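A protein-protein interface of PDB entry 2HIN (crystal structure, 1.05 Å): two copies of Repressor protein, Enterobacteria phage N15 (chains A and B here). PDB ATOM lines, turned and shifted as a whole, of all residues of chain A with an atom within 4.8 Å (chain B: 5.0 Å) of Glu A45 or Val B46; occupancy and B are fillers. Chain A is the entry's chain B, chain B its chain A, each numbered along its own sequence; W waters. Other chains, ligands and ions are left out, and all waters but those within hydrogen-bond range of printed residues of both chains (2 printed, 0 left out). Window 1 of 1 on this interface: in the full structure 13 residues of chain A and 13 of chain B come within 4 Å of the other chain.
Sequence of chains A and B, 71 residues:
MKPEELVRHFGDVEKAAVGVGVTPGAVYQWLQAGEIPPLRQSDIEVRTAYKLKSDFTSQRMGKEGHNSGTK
Of the 17 printed residues of chain A, 9 touch a printed residue of chain B.
Hydrophobic or aromatic side chains of chain A within 4 Å of the printed part of chain B: Val A46, Tyr A50 and Phe A56.
Printed residues of chain B that touch a printed residue of chain A: Ser B42, Asp B43, Glu B45, Val B46, Arg B47 and Tyr B50.
Hydrophobic or aromatic side chains of chain B within 4 Å of the printed part of chain A: Val B46 and Tyr B50.
Among the printed residues, no Asp or Glu carboxylate lies within 4 Å of a Lys or Arg side-chain nitrogen of the other chain.
Water W2 bridges OG1 of Thr A57 and O of Val B46.
Water W1 bridges the side-chain hydroxyl (OG) of Ser A42 and the guanidinium group (NH2) of Arg B47.
OD1 of Asp B43 sits at hydrogen-bond distance from OG of Ser A42, at 2.7 Å.
The side-chain carboxylate (OE2) of Glu A45 is in hydrogen-bond range of the side-chain hydroxyl (OH) of Tyr B50 (2.6 Å).
The side-chain carboxylate (OE2) of Glu B45 sits at hydrogen-bond distance from the side-chain hydroxyl (OH) of Tyr A50 (2.6 Å).
OD1 of Asp A43 sits at hydrogen-bond distance from OG of Ser B42, at 2.7 Å.
Printed residues of chain B within 4 Å of Ser A42: Ser B42 (3.8 Å), Asp B43 (2.7 Å) and Val B46 (3.7 Å).
Of the printed residues of chain B, Asp A43 touches Ser B42.
Of chain B, only Val B46 (3.6 Å) and Tyr B50 (2.6 Å) come within 4 Å of Glu A45.
Of the printed residues of chain B, Val A46 touches Ser B42 and Glu B45.
Lys A51 touches none of the printed residues of chain B.
Of the printed residues of chain A, Asp B43 touches Ser A42 (2.7 Å).
Val B46 touches five residues of chain A.
The nearest printed residue of chain B that does not touch Glu A45 is Glu B45 (6.5 Å).
The nearest residue of chain A that does not touch Val B46 is Val A46 (4.1 Å).
The nearest printed residue of chain B that does not touch Phe A56 is Ala B49 (5.3 Å).
Ser A42 touches Val B46, and with the chains exchanged Val A46 touches Ser B42.
Glu A45 touches Val B46, and with the chains exchanged Val A46 touches Glu B45.
Glu A45 touches Tyr B50, and with the chains exchanged Tyr A50 touches Glu B45.
Tyr B50 touches its own counterpart, Tyr A50.
Positions printed for both chains: 42, 43, 44, 45, 46, 47, 48, 49 and 50.
Ser B42 touches Ser A42 (CB to O, 3.8 Å).
OG of Ser A42 touches CB of Val B46, at 3.7 Å.
Ser B42 touches Val A46.
OH of Tyr A50 touches CD1 of Tyr B50, 3.4 Å away.
Lys A53 touches Tyr B50 (CE to OH, 3.6 Å).
Ser A54 touches Val B46.
Val B46 touches Phe A56.
Arg B47 touches Phe A56 (CA to CZ, 3.6 Å).
Thr A57 touches Val B46.
Tyr B50 touches Thr A57.
The backbone NH of Tyr A50 sits at hydrogen-bond distance from the backbone carbonyl oxygen of Glu A45 (2.8 Å).
O of Tyr A50 is in hydrogen-bond range of NZ of Lys A53 (2.8 Å).
OG1 of Thr A57 is in hydrogen-bond range of OE2 of Glu A45, at 2.7 Å.
The backbone NH (N) of Tyr B50 sits at hydrogen-bond distance from the backbone carbonyl oxygen (O) of Glu B45 (2.8 Å).
O of Glu A45 sits at hydrogen-bond distance from OG1 of Thr A48, 3.3 Å away.
The backbone NH (N) of Met A1 lies within hydrogen-bond range of the backbone carbonyl oxygen (O) of Lys A53 (2.8 Å).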
ATOM      1  N   MET A   1     -12.755 -19.198 -21.902  1.00  0.00           N
ATOM      2  CA  MET A   1     -14.157 -19.062 -21.438  1.00  0.00           C
ATOM      3  C   MET A   1     -15.076 -19.840 -22.361  1.00  0.00           C
ATOM      4  O   MET A   1     -14.846 -19.939 -23.572  1.00  0.00           O
ATOM      5  CB  MET A   1     -14.617 -17.596 -21.337  1.00  0.00           C
ATOM      6  CG  MET A   1     -15.017 -16.884 -22.655  1.00  0.00           C
ATOM      7  SD  MET A   1     -13.712 -16.615 -23.855  1.00  0.00           S
ATOM      8  CE  MET A   1     -12.771 -15.286 -23.130  1.00  0.00           C
ATOM      9  N   GLN A  41     -11.241 -16.375 -28.446  1.00  0.00           N
ATOM     10  CA  GLN A  41     -11.246 -16.213 -26.996  1.00  0.00           C
ATOM     11  C   GLN A  41     -10.271 -15.127 -26.573  1.00  0.00           C
ATOM     12  O   GLN A  41     -10.598 -14.301 -25.725  1.00  0.00           O
ATOM     13  CB  GLN A  41     -10.897 -17.505 -26.262  1.00  0.00           C
ATOM     14  CG  GLN A  41     -11.975 -18.597 -26.340  1.00  0.00           C
ATOM     15  CD  GLN A  41     -11.642 -19.755 -25.453  1.00  0.00           C
ATOM     16  OE1 GLN A  41     -11.246 -19.563 -24.293  1.00  0.00           O
ATOM     17  NE2 GLN A  41     -11.736 -20.972 -25.995  1.00  0.00           N
ATOM     18  N   SER A  42      -9.059 -15.142 -27.121  1.00  0.00           N
ATOM     19  CA  SER A  42      -8.078 -14.112 -26.779  1.00  0.00           C
ATOM     20  C   SER A  42      -8.601 -12.721 -27.076  1.00  0.00           C
ATOM     21  O   SER A  42      -8.398 -11.805 -26.308  1.00  0.00           O
ATOM     22  CB  SER A  42      -6.743 -14.307 -27.477  1.00  0.00           C
ATOM     23  OG  SER A  42      -6.125 -15.484 -27.013  1.00  0.00           O
ATOM     24  N   ASP A  43      -9.268 -12.559 -28.210  1.00  0.00           N
ATOM     25  CA  ASP A  43      -9.788 -11.255 -28.565  1.00  0.00           C
ATOM     26  C   ASP A  43     -10.885 -10.840 -27.592  1.00  0.00           C
ATOM     27  O   ASP A  43     -10.961  -9.661 -27.247  1.00  0.00           O
ATOM     28  CB  ASP A  43     -10.320 -11.254 -29.985  1.00  0.00           C
ATOM     29  CG  ASP A  43     -10.436  -9.855 -30.544  1.00  0.00           C
ATOM     30  OD1 ASP A  43      -9.459  -9.082 -30.503  1.00  0.00           O
ATOM     31  OD2 ASP A  43     -11.528  -9.503 -31.016  1.00  0.00           O
ATOM     32  N   ILE A  44     -11.737 -11.763 -27.169  1.00  0.00           N
ATOM     33  CA  ILE A  44     -12.742 -11.449 -26.153  1.00  0.00           C
ATOM     34  C   ILE A  44     -12.095 -11.014 -24.848  1.00  0.00           C
ATOM     35  O   ILE A  44     -12.519 -10.046 -24.227  1.00  0.00           O
ATOM     36  CB  ILE A  44     -13.678 -12.654 -25.948  1.00  0.00           C
ATOM     37  CG1 ILE A  44     -14.515 -12.903 -27.208  1.00  0.00           C
ATOM     38  CG2 ILE A  44     -14.568 -12.440 -24.720  1.00  0.00           C
ATOM     39  CD1 ILE A  44     -15.193 -14.288 -27.223  1.00  0.00           C
ATOM     40  N   GLU A  45     -11.065 -11.744 -24.434  1.00  0.00           N
ATOM     41  CA  GLU A  45     -10.341 -11.419 -23.212  1.00  0.00           C
ATOM     42  C   GLU A  45      -9.779  -9.991 -23.285  1.00  0.00           C
ATOM     43  O   GLU A  45      -9.947  -9.204 -22.359  1.00  0.00           O
ATOM     44  CB  GLU A  45      -9.251 -12.446 -23.011  1.00  0.00           C
ATOM     45  CG  GLU A  45      -8.384 -12.245 -21.789  1.00  0.00           C
ATOM     46  CD  GLU A  45      -7.463 -13.425 -21.520  1.00  0.00           C
ATOM     47  OE1 GLU A  45      -7.727 -14.515 -22.068  1.00  0.00           O
ATOM     48  OE2 GLU A  45      -6.496 -13.268 -20.720  1.00  0.00           O
ATOM     49  N   VAL A  46      -9.159  -9.635 -24.399  1.00  0.00           N
ATOM     50  CA  VAL A  46      -8.582  -8.320 -24.519  1.00  0.00           C
ATOM     51  C   VAL A  46      -9.683  -7.256 -24.623  1.00  0.00           C
ATOM     52  O   VAL A  46      -9.600  -6.210 -23.979  1.00  0.00           O
ATOM     53  CB  VAL A  46      -7.614  -8.273 -25.743  1.00  0.00           C
ATOM     54  CG1 VAL A  46      -7.245  -6.824 -26.126  1.00  0.00           C
ATOM     55  CG2 VAL A  46      -6.389  -9.112 -25.417  1.00  0.00           C
ATOM     56  N   ARG A  47     -10.716  -7.488 -25.439  1.00  0.00           N
ATOM     57  CA  ARG A  47     -11.731  -6.466 -25.657  1.00  0.00           C
ATOM     58  C   ARG A  47     -12.583  -6.207 -24.423  1.00  0.00           C
ATOM     59  O   ARG A  47     -13.179  -5.143 -24.327  1.00  0.00           O
ATOM     60  CB  ARG A  47     -12.570  -6.786 -26.883  1.00  0.00           C
ATOM     61  CG  ARG A  47     -11.722  -6.592 -28.138  1.00  0.00           C
ATOM     62  CD  ARG A  47     -12.482  -6.612 -29.421  1.00  0.00           C
ATOM     63  NE  ARG A  47     -13.110  -5.331 -29.699  1.00  0.00           N
ATOM     64  CZ  ARG A  47     -12.544  -4.316 -30.359  1.00  0.00           C
ATOM     65  NH1 ARG A  47     -11.310  -4.388 -30.863  1.00  0.00           N
ATOM     66  NH2 ARG A  47     -13.237  -3.207 -30.518  1.00  0.00           N
ATOM     67  N   THR A  48     -12.663  -7.161 -23.499  1.00  0.00           N
ATOM     68  CA  THR A  48     -13.347  -6.995 -22.216  1.00  0.00           C
ATOM     69  C   THR A  48     -12.378  -6.536 -21.119  1.00  0.00           C
ATOM     70  O   THR A  48     -12.752  -6.552 -19.941  1.00  0.00           O
ATOM     71  CB  THR A  48     -14.106  -8.289 -21.792  1.00  0.00           C
ATOM     72  OG1 THR A  48     -13.171  -9.329 -21.496  1.00  0.00           O
ATOM     73  CG2 THR A  48     -15.137  -8.718 -22.847  1.00  0.00           C
ATOM     74  N   ALA A  49     -11.151  -6.139 -21.486  1.00  0.00           N
ATOM     75  CA  ALA A  49     -10.160  -5.692 -20.496  1.00  0.00           C
ATOM     76  C   ALA A  49      -9.971  -6.748 -19.396  1.00  0.00           C
ATOM     77  O   ALA A  49      -9.840  -6.446 -18.214  1.00  0.00           O
ATOM     78  CB  ALA A  49     -10.530  -4.290 -19.949  1.00  0.00           C
ATOM     79  N   TYR A  50      -9.945  -7.987 -19.836  1.00  0.00           N
ATOM     80  CA  TYR A  50      -9.602  -9.163 -19.054  1.00  0.00           C
ATOM     81  C   TYR A  50     -10.723  -9.607 -18.124  1.00  0.00           C
ATOM     82  O   TYR A  50     -10.522 -10.484 -17.290  1.00  0.00           O
ATOM     83  CB  TYR A  50      -8.292  -9.019 -18.262  1.00  0.00           C
ATOM     84  CG  TYR A  50      -7.095  -8.503 -19.039  1.00  0.00           C
ATOM     85  CD1 TYR A  50      -7.008  -8.534 -20.441  1.00  0.00           C
ATOM     86  CD2 TYR A  50      -6.001  -8.007 -18.344  1.00  0.00           C
ATOM     87  CE1 TYR A  50      -5.875  -8.027 -21.093  1.00  0.00           C
ATOM     88  CE2 TYR A  50      -4.884  -7.533 -18.985  1.00  0.00           C
ATOM     89  CZ  TYR A  50      -4.814  -7.521 -20.363  1.00  0.00           C
ATOM     90  OH  TYR A  50      -3.674  -7.049 -20.976  1.00  0.00           O
ATOM     91  N   LYS A  51     -11.924  -9.050 -18.269  1.00  0.00           N
ATOM     92  CA  LYS A  51     -13.053  -9.503 -17.438  1.00  0.00           C
ATOM     93  C   LYS A  51     -13.445 -10.942 -17.736  1.00  0.00           C
ATOM     94  O   LYS A  51     -13.861 -11.655 -16.822  1.00  0.00           O
ATOM     95  CB  LYS A  51     -14.264  -8.599 -17.663  1.00  0.00           C
ATOM     96  CG  LYS A  51     -14.055  -7.177 -17.173  1.00  0.00           C
ATOM     97  CD  LYS A  51     -15.179  -6.279 -17.616  1.00  0.00           C
ATOM     98  CE  LYS A  51     -14.870  -4.822 -17.346  1.00  0.00           C
ATOM     99  NZ  LYS A  51     -13.692  -4.322 -18.151  1.00  0.00           N
ATOM    100  N   LEU A  52     -13.319 -11.354 -18.986  1.00  0.00           N
ATOM    101  CA  LEU A  52     -13.494 -12.752 -19.379  1.00  0.00           C
ATOM    102  C   LEU A  52     -12.119 -13.321 -19.726  1.00  0.00           C
ATOM    103  O   LEU A  52     -11.323 -12.636 -20.390  1.00  0.00           O
ATOM    104  CB  LEU A  52     -14.437 -12.864 -20.569  1.00  0.00           C
ATOM    105  CG  LEU A  52     -15.898 -12.499 -20.288  1.00  0.00           C
ATOM    106  CD1 LEU A  52     -16.678 -12.470 -21.582  1.00  0.00           C
ATOM    107  CD2 LEU A  52     -16.504 -13.482 -19.303  1.00  0.00           C
ATOM    108  N   LYS A  53     -11.853 -14.547 -19.307  1.00  0.00           N
ATOM    109  CA  LYS A  53     -10.548 -15.167 -19.529  1.00  0.00           C
ATOM    110  C   LYS A  53     -10.633 -16.313 -20.498  1.00  0.00           C
ATOM    111  O   LYS A  53     -11.518 -17.192 -20.399  1.00  0.00           O
ATOM    112  CB  LYS A  53     -10.023 -15.723 -18.219  1.00  0.00           C
ATOM    113  CG  LYS A  53      -9.826 -14.670 -17.128  1.00  0.00           C
ATOM    114  CD  LYS A  53      -8.921 -13.524 -17.543  1.00  0.00           C
ATOM    115  CE  LYS A  53      -8.277 -12.818 -16.368  1.00  0.00           C
ATOM    116  NZ  LYS A  53      -9.275 -12.185 -15.453  1.00  0.00           N
ATOM    117  N   SER A  54      -9.697 -16.328 -21.442  1.00  0.00           N
ATOM    118  CA  SER A  54      -9.517 -17.466 -22.308  1.00  0.00           C
ATOM    119  C   SER A  54      -9.162 -18.706 -21.506  1.00  0.00           C
ATOM    120  O   SER A  54      -8.683 -18.627 -20.381  1.00  0.00           O
ATOM    121  CB  SER A  54      -8.411 -17.184 -23.322  1.00  0.00           C
ATOM    122  OG  SER A  54      -7.133 -17.080 -22.656  1.00  0.00           O
ATOM    123  N   PHE A  56      -6.631 -20.512 -22.136  1.00  0.00           N
ATOM    124  CA  PHE A  56      -5.192 -20.332 -21.943  1.00  0.00           C
ATOM    125  C   PHE A  56      -4.916 -19.610 -20.630  1.00  0.00           C
ATOM    126  O   PHE A  56      -4.144 -20.091 -19.785  1.00  0.00           O
ATOM    127  CB  PHE A  56      -4.636 -19.532 -23.127  1.00  0.00           C
ATOM    128  CG  PHE A  56      -3.160 -19.295 -23.084  1.00  0.00           C
ATOM    129  CD1 PHE A  56      -2.315 -20.015 -23.905  1.00  0.00           C
ATOM    130  CD2 PHE A  56      -2.608 -18.341 -22.248  1.00  0.00           C
ATOM    131  CE1 PHE A  56      -0.950 -19.792 -23.889  1.00  0.00           C
ATOM    132  CE2 PHE A  56      -1.232 -18.118 -22.223  1.00  0.00           C
ATOM    133  CZ  PHE A  56      -0.400 -18.857 -23.052  1.00  0.00           C
ATOM    134  N   THR A  57      -5.538 -18.460 -20.444  1.00  0.00           N
ATOM    135  CA  THR A  57      -5.286 -17.668 -19.241  1.00  0.00           C
ATOM    136  C   THR A  57      -5.763 -18.373 -17.998  1.00  0.00           C
ATOM    137  O   THR A  57      -5.107 -18.351 -16.956  1.00  0.00           O
ATOM    138  CB  THR A  57      -5.936 -16.290 -19.369  1.00  0.00           C
ATOM    139  OG1 THR A  57      -5.292 -15.627 -20.468  1.00  0.00           O
ATOM    140  CG2 THR A  57      -5.750 -15.455 -18.086  1.00  0.00           C
ATOM    141  N   SER B  42      -4.279  -9.538 -30.127  1.00  0.00           N
ATOM    142  CA  SER B  42      -4.947  -9.973 -28.902  1.00  0.00           C
ATOM    143  C   SER B  42      -4.392 -11.282 -28.403  1.00  0.00           C
ATOM    144  O   SER B  42      -4.165 -11.468 -27.207  1.00  0.00           O
ATOM    145  CB  SER B  42      -6.465 -10.108 -29.094  1.00  0.00           C
ATOM    146  OG  SER B  42      -7.039  -8.835 -29.273  1.00  0.00           O
ATOM    147  N   ASP B  43      -4.196 -12.210 -29.321  1.00  0.00           N
ATOM    148  CA  ASP B  43      -3.667 -13.522 -28.954  1.00  0.00           C
ATOM    149  C   ASP B  43      -2.236 -13.407 -28.400  1.00  0.00           C
ATOM    150  O   ASP B  43      -1.888 -14.113 -27.457  1.00  0.00           O
ATOM    151  CB  ASP B  43      -3.764 -14.493 -30.113  1.00  0.00           C
ATOM    152  CG  ASP B  43      -3.589 -15.921 -29.676  1.00  0.00           C
ATOM    153  OD1 ASP B  43      -4.306 -16.387 -28.748  1.00  0.00           O
ATOM    154  OD2 ASP B  43      -2.737 -16.634 -30.253  1.00  0.00           O
ATOM    155  N   ILE B  44      -1.416 -12.539 -28.991  1.00  0.00           N
ATOM    156  CA  ILE B  44      -0.054 -12.337 -28.512  1.00  0.00           C
ATOM    157  C   ILE B  44      -0.079 -11.735 -27.107  1.00  0.00           C
ATOM    158  O   ILE B  44       0.709 -12.138 -26.242  1.00  0.00           O
ATOM    159  CB  ILE B  44       0.719 -11.469 -29.505  1.00  0.00           C
ATOM    160  CG1 ILE B  44       0.895 -12.224 -30.826  1.00  0.00           C
ATOM    161  CG2 ILE B  44       2.104 -11.069 -28.933  1.00  0.00           C
ATOM    162  CD1 ILE B  44       1.406 -11.333 -31.969  1.00  0.00           C
ATOM    163  N   GLU B  45      -0.966 -10.778 -26.873  1.00  0.00           N
ATOM    164  CA  GLU B  45      -1.110 -10.185 -25.541  1.00  0.00           C
ATOM    165  C   GLU B  45      -1.455 -11.240 -24.506  1.00  0.00           C
ATOM    166  O   GLU B  45      -0.844 -11.322 -23.445  1.00  0.00           O
ATOM    167  CB  GLU B  45      -2.168  -9.094 -25.607  1.00  0.00           C
ATOM    168  CG  GLU B  45      -2.480  -8.397 -24.299  1.00  0.00           C
ATOM    169  CD  GLU B  45      -3.385  -7.189 -24.485  1.00  0.00           C
ATOM    170  OE1 GLU B  45      -3.447  -6.664 -25.603  1.00  0.00           O
ATOM    171  OE2 GLU B  45      -4.020  -6.714 -23.524  1.00  0.00           O
ATOM    172  N   VAL B  46      -2.407 -12.101 -24.823  1.00  0.00           N
ATOM    173  CA  VAL B  46      -2.807 -13.170 -23.903  1.00  0.00           C
ATOM    174  C   VAL B  46      -1.657 -14.169 -23.737  1.00  0.00           C
ATOM    175  O   VAL B  46      -1.343 -14.566 -22.608  1.00  0.00           O
ATOM    176  CB  VAL B  46      -4.099 -13.857 -24.426  1.00  0.00           C
ATOM    177  CG1 VAL B  46      -4.372 -15.187 -23.688  1.00  0.00           C
ATOM    178  CG2 VAL B  46      -5.279 -12.887 -24.279  1.00  0.00           C
ATOM    179  N   ARG B  47      -1.045 -14.595 -24.826  1.00  0.00           N
ATOM    180  CA  ARG B  47      -0.088 -15.681 -24.764  1.00  0.00           C
ATOM    181  C   ARG B  47       1.282 -15.274 -24.245  1.00  0.00           C
ATOM    182  O   ARG B  47       2.088 -16.148 -23.967  1.00  0.00           O
ATOM    183  CB  ARG B  47      -0.073 -16.428 -26.089  1.00  0.00           C
ATOM    184  CG  ARG B  47      -1.443 -17.101 -26.317  1.00  0.00           C
ATOM    185  CD  ARG B  47      -1.516 -18.093 -27.443  1.00  0.00           C
ATOM    186  NE  ARG B  47      -2.890 -18.590 -27.562  1.00  0.00           N
ATOM    187  CZ  ARG B  47      -3.275 -19.861 -27.515  1.00  0.00           C
ATOM    188  NH1 ARG B  47      -2.400 -20.844 -27.443  1.00  0.00           N
ATOM    189  NH2 ARG B  47      -4.560 -20.138 -27.572  1.00  0.00           N
ATOM    190  N   THR B  48       1.502 -13.980 -24.042  1.00  0.00           N
ATOM    191  CA  THR B  48       2.664 -13.451 -23.318  1.00  0.00           C
ATOM    192  C   THR B  48       2.279 -13.020 -21.904  1.00  0.00           C
ATOM    193  O   THR B  48       3.043 -12.307 -21.242  1.00  0.00           O
ATOM    194  CB  THR B  48       3.348 -12.285 -24.071  1.00  0.00           C
ATOM    195  OG1 THR B  48       2.449 -11.178 -24.178  1.00  0.00           O
ATOM    196  CG2 THR B  48       3.843 -12.709 -25.445  1.00  0.00           C
ATOM    197  N   ALA B  49       1.124 -13.477 -21.416  1.00  0.00           N
ATOM    198  CA  ALA B  49       0.675 -13.169 -20.044  1.00  0.00           C
ATOM    199  C   ALA B  49       0.654 -11.652 -19.824  1.00  0.00           C
ATOM    200  O   ALA B  49       1.006 -11.141 -18.763  1.00  0.00           O
ATOM    201  CB  ALA B  49       1.526 -13.878 -19.031  1.00  0.00           C
ATOM    202  N   TYR B  50       0.246 -10.950 -20.863  1.00  0.00           N
ATOM    203  CA  TYR B  50       0.026  -9.509 -20.889  1.00  0.00           C
ATOM    204  C   TYR B  50       1.307  -8.702 -20.943  1.00  0.00           C
ATOM    205  O   TYR B  50       1.271  -7.477 -20.808  1.00  0.00           O
ATOM    206  CB  TYR B  50      -0.840  -9.040 -19.718  1.00  0.00           C
ATOM    207  CG  TYR B  50      -2.094  -9.858 -19.489  1.00  0.00           C
ATOM    208  CD1 TYR B  50      -2.908 -10.311 -20.529  1.00  0.00           C
ATOM    209  CD2 TYR B  50      -2.486 -10.180 -18.192  1.00  0.00           C
ATOM    210  CE1 TYR B  50      -4.073 -11.031 -20.268  1.00  0.00           C
ATOM    211  CE2 TYR B  50      -3.644 -10.880 -17.936  1.00  0.00           C
ATOM    212  CZ  TYR B  50      -4.443 -11.313 -18.969  1.00  0.00           C
ATOM    213  OH  TYR B  50      -5.636 -11.942 -18.675  1.00  0.00           O
HETATM  214  O   HOH W   1      -6.775 -18.233 -26.616  1.00  0.00           O
HETATM  215  O   HOH W   2      -2.619 -15.213 -20.228  1.00  0.00           O
